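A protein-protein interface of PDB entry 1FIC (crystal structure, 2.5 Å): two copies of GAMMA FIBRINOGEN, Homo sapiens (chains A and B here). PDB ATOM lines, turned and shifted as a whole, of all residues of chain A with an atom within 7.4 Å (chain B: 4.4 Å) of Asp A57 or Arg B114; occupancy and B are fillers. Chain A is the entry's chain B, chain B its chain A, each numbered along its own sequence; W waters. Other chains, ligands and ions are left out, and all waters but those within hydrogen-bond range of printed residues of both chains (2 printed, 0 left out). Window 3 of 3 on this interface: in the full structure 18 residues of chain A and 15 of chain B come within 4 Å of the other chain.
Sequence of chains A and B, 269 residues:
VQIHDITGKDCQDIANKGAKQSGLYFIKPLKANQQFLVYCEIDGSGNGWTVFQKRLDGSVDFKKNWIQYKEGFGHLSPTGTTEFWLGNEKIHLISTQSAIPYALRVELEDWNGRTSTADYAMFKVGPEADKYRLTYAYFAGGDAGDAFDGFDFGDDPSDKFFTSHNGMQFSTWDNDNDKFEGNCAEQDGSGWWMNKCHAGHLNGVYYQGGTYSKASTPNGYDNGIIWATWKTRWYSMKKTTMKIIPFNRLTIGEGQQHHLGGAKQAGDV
Of the 9 printed residues of chain B, 4 touch a printed residue of chain A. Of the 17 printed residues of chain A, 3 touch a printed residue of chain B. Among the printed residues, no Asp or Glu carboxylate lies within 4 Å of a Lys or Arg side-chain nitrogen of the other chain.
Asp A57 touches Arg B114 (CB to NH1, 3.4 Å). Lys B231 touches Ser A59 (CA to O, 3.7 Å).
OD1 of Asp A57 lies within hydrogen-bond range of OG of Ser A59 (2.8 Å). N of Ser A59 sits at hydrogen-bond distance from OE1 of Glu A83 (3.3 Å). N of Asp A57 lies within hydrogen-bond range of OE2 of Glu A83 (2.8 Å). The guanidinium group (NE) of Arg B114 lies within salt-bridge range of the side-chain carboxylate (OD2) of Asp B110 (2.5 Å). OD2 of Asp B110 is in salt-bridge range of NZ of Lys B231 (2.8 Å).
No position is printed for both chains.
Water W1 lies within hydrogen-bond range of NE2 of Gln A208 (2.5 Å) and NH2 of Arg B114 (2.9 Å). Water W2 lies within hydrogen-bond range of the backbone carbonyl oxygen (O) of Asp A57 and the side-chain amino group (NZ) of Lys B231.
NE2 of Gln A208 sits close to ND2 of Asn B112, at 3.5 Å. O of Trp B230 sits close to O of Ser A59, 3.5 Å away.
Arg A55 touches none of the printed residues of chain B. Of chain B, only Arg B114 comes within 4 Å of Asp A57. Of the printed residues of chain B, Ser A59 touches Trp B230 and Lys B231. Of the printed residues of chain B, Gln A208 touches Asn B112. Of the printed residues of chain A, Asn B112 touches Gln A208. Of chain A, only Asp A57 (3.4 Å) comes within 4 Å of Arg B114. Of the printed residues of chain A, Trp B230 touches Ser A59 (3.2 Å). Printed residues of chain A within 4 Å of Lys B231: Ser A59 (3.7 Å). The nearest residue of chain B that does not touch Asp A57 is Lys B231 (4.2 Å). The nearest residue of chain A that does not touch Arg B114 is Gln A208 (4.3 Å).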
ATOM      1  N   LYS A  54     -20.534   9.715  11.922  1.00  0.00           N
ATOM      2  CA  LYS A  54     -21.698  10.256  11.236  1.00  0.00           C
ATOM      3  C   LYS A  54     -21.261  10.984   9.966  1.00  0.00           C
ATOM      4  O   LYS A  54     -20.331  11.764   9.999  1.00  0.00           O
ATOM      5  CB  LYS A  54     -22.442  11.200  12.181  1.00  0.00           C
ATOM      6  CG  LYS A  54     -23.822  11.696  11.709  1.00  0.00           C
ATOM      7  CD  LYS A  54     -24.865  10.636  11.896  1.00  0.00           C
ATOM      8  CE  LYS A  54     -26.242  11.170  11.732  1.00  0.00           C
ATOM      9  NZ  LYS A  54     -27.163  10.068  11.311  1.00  0.00           N
ATOM     10  N   ARG A  55     -21.862  10.659   8.829  1.00  0.00           N
ATOM     11  CA  ARG A  55     -21.519  11.336   7.592  1.00  0.00           C
ATOM     12  C   ARG A  55     -22.843  11.784   7.065  1.00  0.00           C
ATOM     13  O   ARG A  55     -23.809  11.043   7.160  1.00  0.00           O
ATOM     14  CB  ARG A  55     -20.955  10.375   6.538  1.00  0.00           C
ATOM     15  CG  ARG A  55     -19.810   9.536   6.961  1.00  0.00           C
ATOM     16  CD  ARG A  55     -18.627  10.363   7.335  1.00  0.00           C
ATOM     17  NE  ARG A  55     -17.967  10.983   6.188  1.00  0.00           N
ATOM     18  CZ  ARG A  55     -17.362  10.322   5.205  1.00  0.00           C
ATOM     19  NH1 ARG A  55     -17.330   9.004   5.202  1.00  0.00           N
ATOM     20  NH2 ARG A  55     -16.730  10.990   4.249  1.00  0.00           N
ATOM     21  N   LEU A  56     -22.926  12.990   6.536  1.00  0.00           N
ATOM     22  CA  LEU A  56     -24.184  13.402   5.953  1.00  0.00           C
ATOM     23  C   LEU A  56     -24.131  14.484   4.884  1.00  0.00           C
ATOM     24  O   LEU A  56     -25.161  14.814   4.291  1.00  0.00           O
ATOM     25  CB  LEU A  56     -25.216  13.697   7.034  1.00  0.00           C
ATOM     26  CG  LEU A  56     -25.183  14.882   7.980  1.00  0.00           C
ATOM     27  CD1 LEU A  56     -25.678  14.416   9.331  1.00  0.00           C
ATOM     28  CD2 LEU A  56     -23.822  15.436   8.115  1.00  0.00           C
ATOM     29  N   ASP A  57     -22.929  14.950   4.552  1.00  0.00           N
ATOM     30  CA  ASP A  57     -22.781  15.996   3.546  1.00  0.00           C
ATOM     31  C   ASP A  57     -21.358  16.282   3.026  1.00  0.00           C
ATOM     32  O   ASP A  57     -21.151  17.269   2.313  1.00  0.00           O
ATOM     33  CB  ASP A  57     -23.408  17.296   4.056  1.00  0.00           C
ATOM     34  CG  ASP A  57     -22.641  17.910   5.217  1.00  0.00           C
ATOM     35  OD1 ASP A  57     -21.561  17.414   5.588  1.00  0.00           O
ATOM     36  OD2 ASP A  57     -23.129  18.912   5.770  1.00  0.00           O
ATOM     37  N   GLY A  58     -20.386  15.450   3.390  1.00  0.00           N
ATOM     38  CA  GLY A  58     -19.017  15.654   2.932  1.00  0.00           C
ATOM     39  C   GLY A  58     -18.310  16.949   3.332  1.00  0.00           C
ATOM     40  O   GLY A  58     -17.376  17.379   2.651  1.00  0.00           O
ATOM     41  N   SER A  59     -18.712  17.560   4.443  1.00  0.00           N
ATOM     42  CA  SER A  59     -18.080  18.796   4.898  1.00  0.00           C
ATOM     43  C   SER A  59     -16.823  18.549   5.738  1.00  0.00           C
ATOM     44  O   SER A  59     -15.997  19.439   5.917  1.00  0.00           O
ATOM     45  CB  SER A  59     -19.070  19.609   5.712  1.00  0.00           C
ATOM     46  OG  SER A  59     -19.468  18.873   6.854  1.00  0.00           O
ATOM     47  N   VAL A  60     -16.682  17.345   6.270  1.00  0.00           N
ATOM     48  CA  VAL A  60     -15.534  17.003   7.085  1.00  0.00           C
ATOM     49  C   VAL A  60     -14.621  16.066   6.312  1.00  0.00           C
ATOM     50  O   VAL A  60     -15.050  15.017   5.827  1.00  0.00           O
ATOM     51  CB  VAL A  60     -15.982  16.334   8.398  1.00  0.00           C
ATOM     52  CG1 VAL A  60     -14.784  15.796   9.163  1.00  0.00           C
ATOM     53  CG2 VAL A  60     -16.730  17.317   9.231  1.00  0.00           C
ATOM     54  N   THR A  81     -26.710  16.748  13.388  1.00  0.00           N
ATOM     55  CA  THR A  81     -26.671  17.130  11.993  1.00  0.00           C
ATOM     56  C   THR A  81     -25.272  17.540  11.535  1.00  0.00           C
ATOM     57  O   THR A  81     -25.113  18.339  10.626  1.00  0.00           O
ATOM     58  CB  THR A  81     -27.681  18.263  11.730  1.00  0.00           C
ATOM     59  OG1 THR A  81     -27.603  19.242  12.780  1.00  0.00           O
ATOM     60  CG2 THR A  81     -29.094  17.705  11.664  1.00  0.00           C
ATOM     61  N   THR A  82     -24.254  16.963  12.144  1.00  0.00           N
ATOM     62  CA  THR A  82     -22.888  17.289  11.791  1.00  0.00           C
ATOM     63  C   THR A  82     -22.155  15.974  11.647  1.00  0.00           C
ATOM     64  O   THR A  82     -22.584  14.955  12.188  1.00  0.00           O
ATOM     65  CB  THR A  82     -22.213  18.100  12.923  1.00  0.00           C
ATOM     66  OG1 THR A  82     -22.512  17.478  14.175  1.00  0.00           O
ATOM     67  CG2 THR A  82     -22.737  19.530  12.967  1.00  0.00           C
ATOM     68  N   GLU A  83     -21.064  16.007  10.894  1.00  0.00           N
ATOM     69  CA  GLU A  83     -20.235  14.838  10.671  1.00  0.00           C
ATOM     70  C   GLU A  83     -19.140  14.833  11.707  1.00  0.00           C
ATOM     71  O   GLU A  83     -18.656  15.901  12.094  1.00  0.00           O
ATOM     72  CB  GLU A  83     -19.580  14.903   9.298  1.00  0.00           C
ATOM     73  CG  GLU A  83     -20.553  15.041   8.190  1.00  0.00           C
ATOM     74  CD  GLU A  83     -19.945  14.773   6.868  1.00  0.00           C
ATOM     75  OE1 GLU A  83     -18.776  15.139   6.666  1.00  0.00           O
ATOM     76  OE2 GLU A  83     -20.630  14.183   6.015  1.00  0.00           O
ATOM     77  N   TRP A 111     -29.278   7.690  -1.723  1.00  0.00           N
ATOM     78  CA  TRP A 111     -29.467   9.002  -2.297  1.00  0.00           C
ATOM     79  C   TRP A 111     -30.913   9.083  -2.756  1.00  0.00           C
ATOM     80  O   TRP A 111     -31.370  10.120  -3.219  1.00  0.00           O
ATOM     81  CB  TRP A 111     -28.485   9.254  -3.417  1.00  0.00           C
ATOM     82  CG  TRP A 111     -27.152   9.582  -2.860  1.00  0.00           C
ATOM     83  CD1 TRP A 111     -26.170   8.713  -2.541  1.00  0.00           C
ATOM     84  CD2 TRP A 111     -26.666  10.885  -2.529  1.00  0.00           C
ATOM     85  NE1 TRP A 111     -25.085   9.384  -2.029  1.00  0.00           N
ATOM     86  CE2 TRP A 111     -25.364  10.724  -2.012  1.00  0.00           C
ATOM     87  CE3 TRP A 111     -27.204  12.183  -2.628  1.00  0.00           C
ATOM     88  CZ2 TRP A 111     -24.583  11.807  -1.588  1.00  0.00           C
ATOM     89  CZ3 TRP A 111     -26.433  13.261  -2.209  1.00  0.00           C
ATOM     90  CH2 TRP A 111     -25.133  13.063  -1.694  1.00  0.00           C
ATOM     91  N   TYR A 206     -16.724  11.239   0.204  1.00  0.00           N
ATOM     92  CA  TYR A 206     -18.129  11.538  -0.016  1.00  0.00           C
ATOM     93  C   TYR A 206     -18.374  11.964  -1.443  1.00  0.00           C
ATOM     94  O   TYR A 206     -17.886  12.994  -1.885  1.00  0.00           O
ATOM     95  CB  TYR A 206     -18.585  12.649   0.926  1.00  0.00           C
ATOM     96  CG  TYR A 206     -20.091  12.760   1.064  1.00  0.00           C
ATOM     97  CD1 TYR A 206     -20.830  13.513   0.174  1.00  0.00           C
ATOM     98  CD2 TYR A 206     -20.771  12.099   2.092  1.00  0.00           C
ATOM     99  CE1 TYR A 206     -22.199  13.615   0.293  1.00  0.00           C
ATOM    100  CE2 TYR A 206     -22.147  12.189   2.217  1.00  0.00           C
ATOM    101  CZ  TYR A 206     -22.848  12.954   1.314  1.00  0.00           C
ATOM    102  OH  TYR A 206     -24.203  13.107   1.440  1.00  0.00           O
ATOM    103  N   GLN A 208     -21.101  13.129  -4.123  1.00  0.00           N
ATOM    104  CA  GLN A 208     -22.439  13.674  -4.256  1.00  0.00           C
ATOM    105  C   GLN A 208     -23.176  12.862  -5.305  1.00  0.00           C
ATOM    106  O   GLN A 208     -22.597  12.474  -6.327  1.00  0.00           O
ATOM    107  CB  GLN A 208     -22.375  15.133  -4.703  1.00  0.00           C
ATOM    108  CG  GLN A 208     -22.699  16.160  -3.624  1.00  0.00           C
ATOM    109  CD  GLN A 208     -24.192  16.286  -3.367  1.00  0.00           C
ATOM    110  OE1 GLN A 208     -25.008  16.222  -4.292  1.00  0.00           O
ATOM    111  NE2 GLN A 208     -24.555  16.467  -2.108  1.00  0.00           N
ATOM    112  N   ILE A 225     -17.904   5.899   0.047  1.00  0.00           N
ATOM    113  CA  ILE A 225     -18.518   5.352   1.253  1.00  0.00           C
ATOM    114  C   ILE A 225     -19.329   4.143   0.806  1.00  0.00           C
ATOM    115  O   ILE A 225     -20.497   4.284   0.431  1.00  0.00           O
ATOM    116  CB  ILE A 225     -19.444   6.398   1.863  1.00  0.00           C
ATOM    117  CG1 ILE A 225     -18.656   7.683   2.149  1.00  0.00           C
ATOM    118  CG2 ILE A 225     -20.067   5.883   3.125  1.00  0.00           C
ATOM    119  CD1 ILE A 225     -19.542   8.821   2.589  1.00  0.00           C
ATOM    120  N   MET A 237     -22.746   6.140  -0.203  1.00  0.00           N
ATOM    121  CA  MET A 237     -23.953   6.467   0.563  1.00  0.00           C
ATOM    122  C   MET A 237     -24.160   7.958   0.784  1.00  0.00           C
ATOM    123  O   MET A 237     -23.222   8.755   0.690  1.00  0.00           O
ATOM    124  CB  MET A 237     -23.963   5.765   1.939  1.00  0.00           C
ATOM    125  CG  MET A 237     -23.543   4.286   1.971  1.00  0.00           C
ATOM    126  SD  MET A 237     -24.353   3.160   0.812  1.00  0.00           S
ATOM    127  CE  MET A 237     -25.916   3.693   0.923  1.00  0.00           C
ATOM    128  N   LYS A 238     -25.405   8.330   1.053  1.00  0.00           N
ATOM    129  CA  LYS A 238     -25.726   9.713   1.334  1.00  0.00           C
ATOM    130  C   LYS A 238     -25.441  10.022   2.802  1.00  0.00           C
ATOM    131  O   LYS A 238     -24.974  11.121   3.123  1.00  0.00           O
ATOM    132  CB  LYS A 238     -27.188  10.004   1.043  1.00  0.00           C
ATOM    133  CG  LYS A 238     -27.526  11.454   1.245  1.00  0.00           C
ATOM    134  CD  LYS A 238     -28.929  11.762   0.836  1.00  0.00           C
ATOM    135  CE  LYS A 238     -29.110  13.244   0.678  1.00  0.00           C
ATOM    136  NZ  LYS A 238     -30.524  13.514   0.300  1.00  0.00           N
ATOM    137  N   LYS A 239     -25.744   9.055   3.681  1.00  0.00           N
ATOM    138  CA  LYS A 239     -25.530   9.178   5.128  1.00  0.00           C
ATOM    139  C   LYS A 239     -25.167   7.854   5.719  1.00  0.00           C
ATOM    140  O   LYS A 239     -25.642   6.823   5.282  1.00  0.00           O
ATOM    141  CB  LYS A 239     -26.806   9.587   5.857  1.00  0.00           C
ATOM    142  CG  LYS A 239     -27.473  10.833   5.362  1.00  0.00           C
ATOM    143  CD  LYS A 239     -28.731  11.072   6.159  1.00  0.00           C
ATOM    144  CE  LYS A 239     -29.543  12.191   5.543  1.00  0.00           C
ATOM    145  NZ  LYS A 239     -30.933  12.180   6.072  1.00  0.00           N
ATOM    146  N   LEU B 108     -19.916  32.429   1.956  1.00  0.00           N
ATOM    147  CA  LEU B 108     -19.624  31.385   0.987  1.00  0.00           C
ATOM    148  C   LEU B 108     -20.883  30.666   0.534  1.00  0.00           C
ATOM    149  O   LEU B 108     -21.888  30.678   1.245  1.00  0.00           O
ATOM    150  CB  LEU B 108     -18.722  30.358   1.643  1.00  0.00           C
ATOM    151  CG  LEU B 108     -17.477  30.901   2.318  1.00  0.00           C
ATOM    152  CD1 LEU B 108     -16.890  29.887   3.248  1.00  0.00           C
ATOM    153  CD2 LEU B 108     -16.499  31.319   1.261  1.00  0.00           C
ATOM    154  N   GLU B 109     -20.822  30.031  -0.641  1.00  0.00           N
ATOM    155  CA  GLU B 109     -21.939  29.247  -1.139  1.00  0.00           C
ATOM    156  C   GLU B 109     -21.529  27.948  -1.808  1.00  0.00           C
ATOM    157  O   GLU B 109     -20.600  27.889  -2.609  1.00  0.00           O
ATOM    158  CB  GLU B 109     -22.878  30.041  -2.039  1.00  0.00           C
ATOM    159  CG  GLU B 109     -24.159  29.279  -2.352  1.00  0.00           C
ATOM    160  CD  GLU B 109     -25.185  30.085  -3.136  1.00  0.00           C
ATOM    161  OE1 GLU B 109     -25.238  31.328  -2.982  1.00  0.00           O
ATOM    162  OE2 GLU B 109     -25.964  29.465  -3.896  1.00  0.00           O
ATOM    163  N   ASP B 110     -22.212  26.899  -1.376  1.00  0.00           N
ATOM    164  CA  ASP B 110     -22.060  25.528  -1.830  1.00  0.00           C
ATOM    165  C   ASP B 110     -22.546  25.381  -3.245  1.00  0.00           C
ATOM    166  O   ASP B 110     -23.258  26.232  -3.764  1.00  0.00           O
ATOM    167  CB  ASP B 110     -23.013  24.638  -1.016  1.00  0.00           C
ATOM    168  CG  ASP B 110     -22.311  23.573  -0.283  1.00  0.00           C
ATOM    169  OD1 ASP B 110     -21.193  23.211  -0.689  1.00  0.00           O
ATOM    170  OD2 ASP B 110     -22.853  23.104   0.719  1.00  0.00           O
ATOM    171  N   ASN B 112     -24.573  23.185  -3.664  1.00  0.00           N
ATOM    172  CA  ASN B 112     -25.859  22.619  -3.287  1.00  0.00           C
ATOM    173  C   ASN B 112     -26.786  23.675  -2.738  1.00  0.00           C
ATOM    174  O   ASN B 112     -27.810  23.352  -2.172  1.00  0.00           O
ATOM    175  CB  ASN B 112     -25.677  21.525  -2.244  1.00  0.00           C
ATOM    176  CG  ASN B 112     -25.850  20.149  -2.825  1.00  0.00           C
ATOM    177  OD1 ASN B 112     -26.933  19.543  -2.733  1.00  0.00           O
ATOM    178  ND2 ASN B 112     -24.798  19.646  -3.465  1.00  0.00           N
ATOM    179  N   GLY B 113     -26.409  24.940  -2.867  1.00  0.00           N
ATOM    180  CA  GLY B 113     -27.256  26.011  -2.385  1.00  0.00           C
ATOM    181  C   GLY B 113     -27.128  26.343  -0.915  1.00  0.00           C
ATOM    182  O   GLY B 113     -27.944  27.102  -0.384  1.00  0.00           O
ATOM    183  N   ARG B 114     -26.126  25.784  -0.244  1.00  0.00           N
ATOM    184  CA  ARG B 114     -25.931  26.079   1.151  1.00  0.00           C
ATOM    185  C   ARG B 114     -25.031  27.297   1.265  1.00  0.00           C
ATOM    186  O   ARG B 114     -24.068  27.445   0.520  1.00  0.00           O
ATOM    187  CB  ARG B 114     -25.307  24.882   1.865  1.00  0.00           C
ATOM    188  CG  ARG B 114     -26.296  23.750   2.139  1.00  0.00           C
ATOM    189  CD  ARG B 114     -25.610  22.426   2.517  1.00  0.00           C
ATOM    190  NE  ARG B 114     -24.925  21.831   1.367  1.00  0.00           N
ATOM    191  CZ  ARG B 114     -24.629  20.540   1.230  1.00  0.00           C
ATOM    192  NH1 ARG B 114     -24.961  19.668   2.170  1.00  0.00           N
ATOM    193  NH2 ARG B 114     -23.984  20.126   0.145  1.00  0.00           N
ATOM    194  N   THR B 115     -25.362  28.185   2.187  1.00  0.00           N
ATOM    195  CA  THR B 115     -24.563  29.374   2.406  1.00  0.00           C
ATOM    196  C   THR B 115     -24.098  29.360   3.866  1.00  0.00           C
ATOM    197  O   THR B 115     -24.756  28.763   4.715  1.00  0.00           O
ATOM    198  CB  THR B 115     -25.375  30.651   2.141  1.00  0.00           C
ATOM    199  OG1 THR B 115     -26.522  30.662   2.997  1.00  0.00           O
ATOM    200  CG2 THR B 115     -25.842  30.702   0.695  1.00  0.00           C
ATOM    201  N   TRP B 230     -15.273  24.680   6.523  1.00  0.00           N
ATOM    202  CA  TRP B 230     -16.653  24.421   6.143  1.00  0.00           C
ATOM    203  C   TRP B 230     -16.706  23.230   5.207  1.00  0.00           C
ATOM    204  O   TRP B 230     -17.622  22.434   5.294  1.00  0.00           O
ATOM    205  CB  TRP B 230     -17.248  25.646   5.451  1.00  0.00           C
ATOM    206  CG  TRP B 230     -18.721  25.617   5.330  1.00  0.00           C
ATOM    207  CD1 TRP B 230     -19.595  25.307   6.309  1.00  0.00           C
ATOM    208  CD2 TRP B 230     -19.510  25.887   4.145  1.00  0.00           C
ATOM    209  NE1 TRP B 230     -20.879  25.357   5.825  1.00  0.00           N
ATOM    210  CE2 TRP B 230     -20.857  25.708   4.498  1.00  0.00           C
ATOM    211  CE3 TRP B 230     -19.205  26.256   2.827  1.00  0.00           C
ATOM    212  CZ2 TRP B 230     -21.912  25.884   3.580  1.00  0.00           C
ATOM    213  CZ3 TRP B 230     -20.251  26.429   1.914  1.00  0.00           C
ATOM    214  CH2 TRP B 230     -21.587  26.242   2.297  1.00  0.00           C
ATOM    215  N   LYS B 231     -15.743  23.133   4.289  1.00  0.00           N
ATOM    216  CA  LYS B 231     -15.688  22.038   3.321  1.00  0.00           C
ATOM    217  C   LYS B 231     -14.259  21.521   3.181  1.00  0.00           C
ATOM    218  O   LYS B 231     -13.308  22.206   3.514  1.00  0.00           O
ATOM    219  CB  LYS B 231     -16.150  22.506   1.942  1.00  0.00           C
ATOM    220  CG  LYS B 231     -17.562  23.048   1.854  1.00  0.00           C
ATOM    221  CD  LYS B 231     -18.587  21.950   1.957  1.00  0.00           C
ATOM    222  CE  LYS B 231     -19.970  22.529   1.880  1.00  0.00           C
ATOM    223  NZ  LYS B 231     -20.990  21.463   1.905  1.00  0.00           N
HETATM  224  O   HOH W   1     -24.105  17.266   0.200  1.00  0.00           O
HETATM  225  O   HOH W   2     -19.982  19.089   0.326  1.00  0.00           O
